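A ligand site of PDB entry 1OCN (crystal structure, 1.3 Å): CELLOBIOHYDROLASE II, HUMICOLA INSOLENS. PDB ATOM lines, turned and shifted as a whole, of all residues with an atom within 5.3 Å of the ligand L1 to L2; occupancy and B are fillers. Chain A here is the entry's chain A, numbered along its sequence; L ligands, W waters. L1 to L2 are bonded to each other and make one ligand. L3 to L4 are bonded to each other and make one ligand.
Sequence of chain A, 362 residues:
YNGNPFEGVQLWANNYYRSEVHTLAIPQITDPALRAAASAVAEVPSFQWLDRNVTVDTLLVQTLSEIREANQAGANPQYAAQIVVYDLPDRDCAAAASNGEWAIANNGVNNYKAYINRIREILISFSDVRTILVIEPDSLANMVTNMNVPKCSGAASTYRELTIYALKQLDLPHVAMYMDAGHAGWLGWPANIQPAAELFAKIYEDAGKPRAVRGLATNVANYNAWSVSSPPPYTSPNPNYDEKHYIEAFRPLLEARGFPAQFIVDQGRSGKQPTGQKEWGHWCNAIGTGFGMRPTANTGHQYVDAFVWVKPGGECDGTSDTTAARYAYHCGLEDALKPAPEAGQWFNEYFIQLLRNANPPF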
ATOM      1  N   TRP A  49      -0.868 -21.289  19.030  1.00  0.00           N
ATOM      2  CA  TRP A  49       0.290 -21.919  19.632  1.00  0.00           C
ATOM      3  C   TRP A  49       0.161 -23.442  19.691  1.00  0.00           C
ATOM      4  O   TRP A  49      -0.793 -23.965  20.236  1.00  0.00           O
ATOM      5  CB  TRP A  49       0.530 -21.367  21.035  1.00  0.00           C
ATOM      6  CG  TRP A  49       0.970 -19.913  21.043  1.00  0.00           C
ATOM      7  CD1 TRP A  49       0.270 -18.834  20.560  1.00  0.00           C
ATOM      8  CD2 TRP A  49       2.170 -19.415  21.568  1.00  0.00           C
ATOM      9  NE1 TRP A  49       0.979 -17.678  20.788  1.00  0.00           N
ATOM     10  CE2 TRP A  49       2.165 -18.005  21.401  1.00  0.00           C
ATOM     11  CE3 TRP A  49       3.266 -19.999  22.201  1.00  0.00           C
ATOM     12  CZ2 TRP A  49       3.163 -17.194  21.878  1.00  0.00           C
ATOM     13  CZ3 TRP A  49       4.302 -19.180  22.651  1.00  0.00           C
ATOM     14  CH2 TRP A  49       4.253 -17.797  22.464  1.00  0.00           C
ATOM     15  N   ASP A  51       1.582 -25.543  21.709  1.00  0.00           N
ATOM     16  CA  ASP A  51       2.287 -25.585  23.001  1.00  0.00           C
ATOM     17  C   ASP A  51       2.308 -26.942  23.661  1.00  0.00           C
ATOM     18  O   ASP A  51       2.961 -27.138  24.671  1.00  0.00           O
ATOM     19  CB  ASP A  51       1.714 -24.556  23.983  1.00  0.00           C
ATOM     20  CG  ASP A  51       0.318 -24.895  24.456  1.00  0.00           C
ATOM     21  OD1 ASP A  51      -0.505 -25.243  23.613  1.00  0.00           O
ATOM     22  OD2 ASP A  51       0.038 -24.859  25.679  1.00  0.00           O
ATOM     23  N   TYR A  86       6.155 -24.347  19.823  1.00  0.00           N
ATOM     24  CA  TYR A  86       6.554 -24.045  21.197  1.00  0.00           C
ATOM     25  C   TYR A  86       6.467 -25.277  22.062  1.00  0.00           C
ATOM     26  O   TYR A  86       5.603 -25.366  22.905  1.00  0.00           O
ATOM     27  CB  TYR A  86       5.715 -22.890  21.735  1.00  0.00           C
ATOM     28  CG  TYR A  86       6.136 -22.405  23.117  1.00  0.00           C
ATOM     29  CD1 TYR A  86       7.391 -21.848  23.319  1.00  0.00           C
ATOM     30  CD2 TYR A  86       5.265 -22.461  24.197  1.00  0.00           C
ATOM     31  CE1 TYR A  86       7.797 -21.423  24.518  1.00  0.00           C
ATOM     32  CE2 TYR A  86       5.694 -21.993  25.450  1.00  0.00           C
ATOM     33  CZ  TYR A  86       6.928 -21.460  25.614  1.00  0.00           C
ATOM     34  OH  TYR A  86       7.337 -21.043  26.874  1.00  0.00           O
ATOM     35  N   ARG A  91      11.713 -26.755  28.147  1.00  0.00           N
ATOM     36  CA  ARG A  91      11.213 -25.476  27.665  1.00  0.00           C
ATOM     37  C   ARG A  91      11.341 -24.416  28.745  1.00  0.00           C
ATOM     38  O   ARG A  91      11.262 -24.729  29.932  1.00  0.00           O
ATOM     39  CB  ARG A  91       9.768 -25.650  27.238  1.00  0.00           C
ATOM     40  CG  ARG A  91       9.220 -24.530  26.357  1.00  0.00           C
ATOM     41  CD  ARG A  91       7.852 -24.849  25.863  1.00  0.00           C
ATOM     42  NE  ARG A  91       6.883 -24.781  26.962  1.00  0.00           N
ATOM     43  CZ  ARG A  91       5.606 -25.151  26.851  1.00  0.00           C
ATOM     44  NH1 ARG A  91       5.113 -25.616  25.731  1.00  0.00           N
ATOM     45  NH2 ARG A  91       4.810 -25.068  27.920  1.00  0.00           N
ATOM     46  N   ASP A  92      11.440 -23.165  28.331  1.00  0.00           N
ATOM     47  CA  ASP A  92      11.369 -22.008  29.243  1.00  0.00           C
ATOM     48  C   ASP A  92      12.418 -22.163  30.343  1.00  0.00           C
ATOM     49  O   ASP A  92      12.150 -22.025  31.530  1.00  0.00           O
ATOM     50  CB  ASP A  92       9.948 -21.842  29.791  1.00  0.00           C
ATOM     51  CG  ASP A  92       9.689 -20.502  30.392  1.00  0.00           C
ATOM     52  OD1 ASP A  92      10.169 -19.462  29.905  1.00  0.00           O
ATOM     53  OD2 ASP A  92       8.924 -20.426  31.377  1.00  0.00           O
ATOM     54  N   SER A  98       6.343 -21.530  32.352  1.00  0.00           N
ATOM     55  CA  SER A  98       5.909 -22.220  31.142  1.00  0.00           C
ATOM     56  C   SER A  98       6.715 -23.485  30.884  1.00  0.00           C
ATOM     57  O   SER A  98       6.861 -23.917  29.746  1.00  0.00           O
ATOM     58  CB  SER A  98       5.914 -21.286  29.923  1.00  0.00           C
ATOM     59  OG  SER A  98       4.856 -20.380  30.001  1.00  0.00           O
ATOM     60  N   PRO A 137       9.656 -19.318  20.830  1.00  0.00           N
ATOM     61  CA  PRO A 137       9.859 -18.169  21.689  1.00  0.00           C
ATOM     62  C   PRO A 137      10.771 -18.444  22.875  1.00  0.00           C
ATOM     63  O   PRO A 137      10.638 -19.467  23.557  1.00  0.00           O
ATOM     64  CB  PRO A 137       8.461 -17.814  22.133  1.00  0.00           C
ATOM     65  CG  PRO A 137       7.633 -18.148  20.920  1.00  0.00           C
ATOM     66  CD  PRO A 137       8.230 -19.433  20.451  1.00  0.00           C
ATOM     67  N   ASP A 138      11.655 -17.481  23.099  1.00  0.00           N
ATOM     68  CA  ASP A 138      12.609 -17.380  24.223  1.00  0.00           C
ATOM     69  C   ASP A 138      13.856 -18.251  24.141  1.00  0.00           C
ATOM     70  O   ASP A 138      14.827 -17.995  24.830  1.00  0.00           O
ATOM     71  CB  ASP A 138      11.971 -17.650  25.575  1.00  0.00           C
ATOM     72  CG  ASP A 138      10.767 -16.737  25.877  1.00  0.00           C
ATOM     73  OD1 ASP A 138      10.789 -15.566  25.449  1.00  0.00           O
ATOM     74  OD2 ASP A 138       9.800 -17.171  26.529  1.00  0.00           O
ATOM     75  N   VAL A 220       7.730 -11.000  21.440  1.00  0.00           N
ATOM     76  CA  VAL A 220       6.741 -12.017  21.674  1.00  0.00           C
ATOM     77  C   VAL A 220       6.450 -12.163  23.157  1.00  0.00           C
ATOM     78  O   VAL A 220       7.345 -12.425  23.962  1.00  0.00           O
ATOM     79  CB  VAL A 220       7.148 -13.360  21.036  1.00  0.00           C
ATOM     80  CG1 VAL A 220       6.163 -14.489  21.385  1.00  0.00           C
ATOM     81  CG2 VAL A 220       7.268 -13.249  19.516  1.00  0.00           C
ATOM     82  N   ALA A 221       5.166 -12.036  23.482  1.00  0.00           N
ATOM     83  CA  ALA A 221       4.724 -12.097  24.857  1.00  0.00           C
ATOM     84  C   ALA A 221       5.267 -11.004  25.756  1.00  0.00           C
ATOM     85  O   ALA A 221       5.187 -11.103  26.981  1.00  0.00           O
ATOM     86  CB  ALA A 221       4.891 -13.481  25.485  1.00  0.00           C
ATOM     87  N   ARG A 269      -0.016  -6.737  23.256  1.00  0.00           N
ATOM     88  CA  ARG A 269      -0.157  -6.167  24.586  1.00  0.00           C
ATOM     89  C   ARG A 269       0.660  -4.870  24.764  1.00  0.00           C
ATOM     90  O   ARG A 269       1.067  -4.518  25.871  1.00  0.00           O
ATOM     91  CB  ARG A 269       0.183  -7.208  25.676  1.00  0.00           C
ATOM     92  CG  ARG A 269      -0.646  -8.449  25.586  1.00  0.00           C
ATOM     93  CD  ARG A 269      -0.549  -9.401  26.763  1.00  0.00           C
ATOM     94  NE  ARG A 269       0.778 -10.015  26.848  1.00  0.00           N
ATOM     95  CZ  ARG A 269       1.190 -10.792  27.846  1.00  0.00           C
ATOM     96  NH1 ARG A 269       0.369 -11.072  28.857  1.00  0.00           N
ATOM     97  NH2 ARG A 269       2.430 -11.230  27.871  1.00  0.00           N
ATOM     98  N   TRP A 283       8.030  -9.545  33.356  1.00  0.00           N
ATOM     99  CA  TRP A 283       7.329 -10.023  32.171  1.00  0.00           C
ATOM    100  C   TRP A 283       5.961 -10.631  32.438  1.00  0.00           C
ATOM    101  O   TRP A 283       5.194 -10.851  31.497  1.00  0.00           O
ATOM    102  CB  TRP A 283       8.188 -11.099  31.406  1.00  0.00           C
ATOM    103  CG  TRP A 283       8.708 -12.149  32.283  1.00  0.00           C
ATOM    104  CD1 TRP A 283       9.904 -12.161  32.899  1.00  0.00           C
ATOM    105  CD2 TRP A 283       8.030 -13.336  32.712  1.00  0.00           C
ATOM    106  NE1 TRP A 283      10.001 -13.246  33.729  1.00  0.00           N
ATOM    107  CE2 TRP A 283       8.863 -13.995  33.614  1.00  0.00           C
ATOM    108  CE3 TRP A 283       6.807 -13.899  32.416  1.00  0.00           C
ATOM    109  CZ2 TRP A 283       8.482 -15.173  34.254  1.00  0.00           C
ATOM    110  CZ3 TRP A 283       6.410 -15.066  33.059  1.00  0.00           C
ATOM    111  CH2 TRP A 283       7.231 -15.672  33.975  1.00  0.00           C
ATOM    112  N   LYS A 311       1.545 -13.461  21.134  1.00  0.00           N
ATOM    113  CA  LYS A 311       0.947 -13.859  22.412  1.00  0.00           C
ATOM    114  C   LYS A 311      -0.525 -13.400  22.425  1.00  0.00           C
ATOM    115  O   LYS A 311      -0.774 -12.217  22.238  1.00  0.00           O
ATOM    116  CB  LYS A 311       1.727 -13.248  23.553  1.00  0.00           C
ATOM    117  CG  LYS A 311       1.061 -13.381  24.931  1.00  0.00           C
ATOM    118  CD  LYS A 311       1.047 -14.816  25.434  1.00  0.00           C
ATOM    119  CE  LYS A 311       0.216 -14.934  26.674  1.00  0.00           C
ATOM    120  NZ  LYS A 311       0.361 -16.272  27.282  1.00  0.00           N
ATOM    121  N   PRO A 312      -1.481 -14.332  22.590  1.00  0.00           N
ATOM    122  CA  PRO A 312      -2.893 -13.940  22.567  1.00  0.00           C
ATOM    123  C   PRO A 312      -3.312 -13.362  23.919  1.00  0.00           C
ATOM    124  O   PRO A 312      -3.366 -14.048  24.923  1.00  0.00           O
ATOM    125  CB  PRO A 312      -3.608 -15.233  22.229  1.00  0.00           C
ATOM    126  CG  PRO A 312      -2.567 -16.160  21.760  1.00  0.00           C
ATOM    127  CD  PRO A 312      -1.372 -15.794  22.613  1.00  0.00           C
ATOM    128  N   GLU A 315      -4.633 -14.930  27.547  1.00  0.00           N
ATOM    129  CA  GLU A 315      -4.012 -16.189  27.936  1.00  0.00           C
ATOM    130  C   GLU A 315      -2.867 -15.851  28.914  1.00  0.00           C
ATOM    131  O   GLU A 315      -2.004 -15.024  28.644  1.00  0.00           O
ATOM    132  CB  GLU A 315      -3.526 -16.988  26.713  1.00  0.00           C
ATOM    133  CG  GLU A 315      -4.681 -17.360  25.829  1.00  0.00           C
ATOM    134  CD  GLU A 315      -4.304 -18.132  24.557  1.00  0.00           C
ATOM    135  OE1 GLU A 315      -3.110 -18.448  24.364  1.00  0.00           O
ATOM    136  OE2 GLU A 315      -5.220 -18.389  23.745  1.00  0.00           O
ATOM    137  N   CYS A 316      -2.883 -16.475  30.082  1.00  0.00           N
ATOM    138  CA  CYS A 316      -2.035 -16.123  31.186  1.00  0.00           C
ATOM    139  C   CYS A 316      -0.544 -16.365  30.901  1.00  0.00           C
ATOM    140  O   CYS A 316      -0.201 -17.246  30.075  1.00  0.00           O
ATOM    141  CB  CYS A 316      -2.459 -16.947  32.407  1.00  0.00           C
ATOM    142  SG  CYS A 316      -1.766 -16.328  33.930  1.00  0.00           S
ATOM    143  N   ASP A 317       0.315 -15.620  31.542  1.00  0.00           N
ATOM    144  CA  ASP A 317       1.762 -15.805  31.457  1.00  0.00           C
ATOM    145  C   ASP A 317       2.312 -16.741  32.553  1.00  0.00           C
ATOM    146  O   ASP A 317       3.469 -17.126  32.506  1.00  0.00           O
ATOM    147  CB  ASP A 317       2.517 -14.502  31.592  1.00  0.00           C
ATOM    148  CG  ASP A 317       2.136 -13.501  30.562  1.00  0.00           C
ATOM    149  OD1 ASP A 317       2.049 -13.858  29.373  1.00  0.00           O
ATOM    150  OD2 ASP A 317       1.978 -12.318  30.876  1.00  0.00           O
ATOM    151  N   ARG A 326       4.947 -24.658  38.872  1.00  0.00           N
ATOM    152  CA  ARG A 326       5.341 -23.696  37.842  1.00  0.00           C
ATOM    153  C   ARG A 326       5.269 -22.271  38.360  1.00  0.00           C
ATOM    154  O   ARG A 326       5.187 -21.354  37.558  1.00  0.00           O
ATOM    155  CB  ARG A 326       4.530 -23.894  36.553  1.00  0.00           C
ATOM    156  CG  ARG A 326       4.673 -25.261  35.929  1.00  0.00           C
ATOM    157  CD  ARG A 326       4.358 -25.279  34.449  1.00  0.00           C
ATOM    158  NE  ARG A 326       3.034 -24.773  34.180  1.00  0.00           N
ATOM    159  CZ  ARG A 326       2.625 -24.433  32.970  1.00  0.00           C
ATOM    160  NH1 ARG A 326       3.390 -24.661  31.913  1.00  0.00           N
ATOM    161  NH2 ARG A 326       1.437 -23.868  32.816  1.00  0.00           N
ATOM    162  N   ALA A 343       0.011 -20.672  33.230  1.00  0.00           N
ATOM    163  CA  ALA A 343       0.391 -20.105  31.926  1.00  0.00           C
ATOM    164  C   ALA A 343      -0.358 -20.828  30.840  1.00  0.00           C
ATOM    165  O   ALA A 343      -0.468 -22.050  30.846  1.00  0.00           O
ATOM    166  CB  ALA A 343       1.896 -20.264  31.706  1.00  0.00           C
ATOM    167  N   GLY A 344      -0.912 -20.030  29.924  1.00  0.00           N
ATOM    168  CA  GLY A 344      -1.652 -20.526  28.806  1.00  0.00           C
ATOM    169  C   GLY A 344      -3.155 -20.648  29.044  1.00  0.00           C
ATOM    170  O   GLY A 344      -3.932 -20.694  28.087  1.00  0.00           O
HETATM  171  O1  LIG L   1       3.327 -18.705  27.780  1.00  0.00           O
HETATM  172  C1  LIG L   1       4.184 -17.671  27.286  1.00  0.00           C
HETATM  173  C2  LIG L   1       4.100 -16.580  28.325  1.00  0.00           C
HETATM  174  O2  LIG L   1       3.002 -15.772  27.949  1.00  0.00           O
HETATM  175  C3  LIG L   1       5.362 -15.780  28.406  1.00  0.00           C
HETATM  176  N1  LIG L   1       6.448 -16.680  28.870  1.00  0.00           N
HETATM  177  C4  LIG L   1       6.544 -17.959  28.185  1.00  0.00           C
HETATM  178  C5  LIG L   1       5.580 -18.257  27.039  1.00  0.00           C
HETATM  179  C6  LIG L   1       6.220 -17.859  25.710  1.00  0.00           C
HETATM  180  O3  LIG L   1       6.165 -16.487  25.531  1.00  0.00           O
HETATM  181  C1  LG2 L   2       2.104 -20.691  27.493  1.00  0.00           C
HETATM  182  C2  LG2 L   2       1.405 -21.555  26.473  1.00  0.00           C
HETATM  183  C3  LG2 L   2       0.512 -20.765  25.563  1.00  0.00           C
HETATM  184  C4  LG2 L   2       1.187 -19.490  25.054  1.00  0.00           C
HETATM  185  C5  LG2 L   2       0.237 -18.519  24.377  1.00  0.00           C
HETATM  186  C6  LG2 L   2       2.762 -19.500  26.805  1.00  0.00           C
HETATM  187  O1  LG2 L   2       3.089 -21.445  28.199  1.00  0.00           O
HETATM  188  O2  LG2 L   2       0.692 -22.569  27.155  1.00  0.00           O
HETATM  189  O3  LG2 L   2       0.137 -21.595  24.483  1.00  0.00           O
HETATM  190  O4  LG2 L   2       1.761 -18.761  26.146  1.00  0.00           O
HETATM  191  O5  LG2 L   2      -0.698 -18.025  25.302  1.00  0.00           O
HETATM  192  O1  LG3 L   3      12.545 -12.969  30.775  1.00  0.00           O
HETATM  193  C1  LG3 L   3      13.537 -12.093  30.255  1.00  0.00           C
HETATM  194  C2  LG3 L   3      13.047 -10.652  30.335  1.00  0.00           C
HETATM  195  O2  LG3 L   3      12.001 -10.385  29.442  1.00  0.00           O
HETATM  196  C3  LG3 L   3      14.161  -9.689  29.957  1.00  0.00           C
HETATM  197  N1  LG3 L   3      15.291  -9.862  30.847  1.00  0.00           N
HETATM  198  C4  LG3 L   3      15.885 -11.186  30.720  1.00  0.00           C
HETATM  199  C5  LG3 L   3      14.817 -12.256  31.061  1.00  0.00           C
HETATM  200  C6  LG3 L   3      15.292 -13.707  31.008  1.00  0.00           C
HETATM  201  O3  LG3 L   3      16.401 -13.902  31.934  1.00  0.00           O
HETATM  202  C1  LG4 L   4      11.135 -14.893  30.581  1.00  0.00           C
HETATM  203  C2  LG4 L   4      10.249 -15.661  29.580  1.00  0.00           C
HETATM  204  C3  LG4 L   4       9.323 -14.647  28.873  1.00  0.00           C
HETATM  205  C4  LG4 L   4      10.088 -13.491  28.264  1.00  0.00           C
HETATM  206  C5  LG4 L   4       9.153 -12.463  27.696  1.00  0.00           C
HETATM  207  C6  LG4 L   4      11.785 -13.769  29.802  1.00  0.00           C
HETATM  208  O1  LG4 L   4      12.126 -15.798  31.070  1.00  0.00           O
HETATM  209  O2  LG4 L   4       9.480 -16.665  30.231  1.00  0.00           O
HETATM  210  O3  LG4 L   4       8.516 -15.319  27.912  1.00  0.00           O
HETATM  211  O4  LG4 L   4      10.831 -12.856  29.285  1.00  0.00           O
HETATM  212  O5  LG4 L   4       9.835 -11.363  27.088  1.00  0.00           O
HETATM  213  O   HOH W   1       5.478 -12.655  29.268  1.00  0.00           O
HETATM  214  O   HOH W   2       8.285 -15.111  24.361  1.00  0.00           O
HETATM  215  O   HOH W   3       2.169 -23.652  29.638  1.00  0.00           O
HETATM  216  O   HOH W   4      -2.435 -20.943  23.643  1.00  0.00           O
HETATM  217  O   HOH W   5       5.617 -18.050  31.181  1.00  0.00           O
HETATM  218  O   HOH W   6       1.907 -25.626  27.630  1.00  0.00           O
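A nitrogen (N1) of LIG L1 is in hydrogen-bond range of an oxygen (O3) of LG4 L4, 2.7 Å away.
O of Tyr 86 is in hydrogen-bond range of NH1 of Arg 91, 2.9 Å away. The side-chain carboxylate of Asp 317 is in salt-bridge range of the guanidinium group of Arg 269 (2.9 Å). The side-chain carboxylate of Asp 317 is in salt-bridge range of the side-chain amino group of Lys 311, 3.6 Å away. OD2 of Asp 92 is in hydrogen-bond range of N of Ser 98, at 3.0 Å. The guanidinium group of Arg 326 is in hydrogen-bond range of the backbone carbonyl oxygen of Ala 343 (3.3 Å). The backbone carbonyl oxygen (O) of Ser 98 is in hydrogen-bond range of the guanidinium group (NE) of Arg 91, 2.9 Å away. The backbone carbonyl oxygen of Asp 51 is in hydrogen-bond range of the guanidinium group of Arg 91, at 2.8 Å. O of Cys 316 is in hydrogen-bond range of NZ of Lys 311 (3.0 Å).
The side-chain carboxylate (OE1) of Glu 315 lies within hydrogen-bond range of an oxygen (O5) of LG2 L2 (2.6 Å). OD1 of Asp 92 lies within hydrogen-bond range of O2 of LG4 L4 (2.9 Å). OD2 of Asp 138 sits at hydrogen-bond distance from O3 of LG4 L4, 2.6 Å away. O1 of LG2 L2 lies within hydrogen-bond range of OG of Ser 98 (2.7 Å). OD1 of Asp 317 lies within hydrogen-bond range of O2 of LIG L1, 2.6 Å away. An oxygen (O2) of LG2 L2 sits at hydrogen-bond distance from the side-chain carboxylate (OD2) of Asp 51. The side-chain amino group (NZ) of Lys 311 lies within hydrogen-bond range of an oxygen (O2) of LIG L1 (2.8 Å).
Water W4 bridges the side-chain carboxylate of Glu 315 and an oxygen (O3) of LG2 L2. Water W2 lies within hydrogen-bond range of the side-chain carboxylate of Asp 138 (2.8 Å), an oxygen (O3) of LIG L1 (2.8 Å) and the backbone carbonyl oxygen of Val 220 (2.9 Å). Water W3 lies within hydrogen-bond range of NH1 of Arg 326 (2.8 Å), O1 of LG2 L2 (2.8 Å), O of Ala 343 (3.3 Å) and NH2 of Arg 91 (3.5 Å). Water W5 lies within hydrogen-bond range of the backbone carbonyl oxygen of Asp 317 (2.7 Å), the side-chain hydroxyl of Ser 98 (2.7 Å) and a nitrogen (N1) of LIG L1 (2.8 Å). Water W1 bridges the backbone carbonyl oxygen of Ala 221 (2.8 Å) and the backbone carbonyl oxygen of Trp 283 (2.9 Å). Water W6 lies within hydrogen-bond range of OD2 of Asp 51 (2.8 Å), NH2 of Arg 91 (3.0 Å) and O2 of LG2 L2 (3.3 Å).
Residues that only touch the ligand L1 to L2: Trp 49 (3.5 Å), Tyr 86 (3.3 Å), Asp 138 (3.7 Å), Ala 221 (3.3 Å), Pro 312 (3.6 Å), Ala 343 (3.9 Å) and Gly 344 (3.5 Å). Within 4 Å of the ligand L1 to L2: Trp 49, Asp 51, Tyr 86, Ser 98, Asp 138, Ala 221, Lys 311, Pro 312, Glu 315, Asp 317, Ala 343 and Gly 344.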
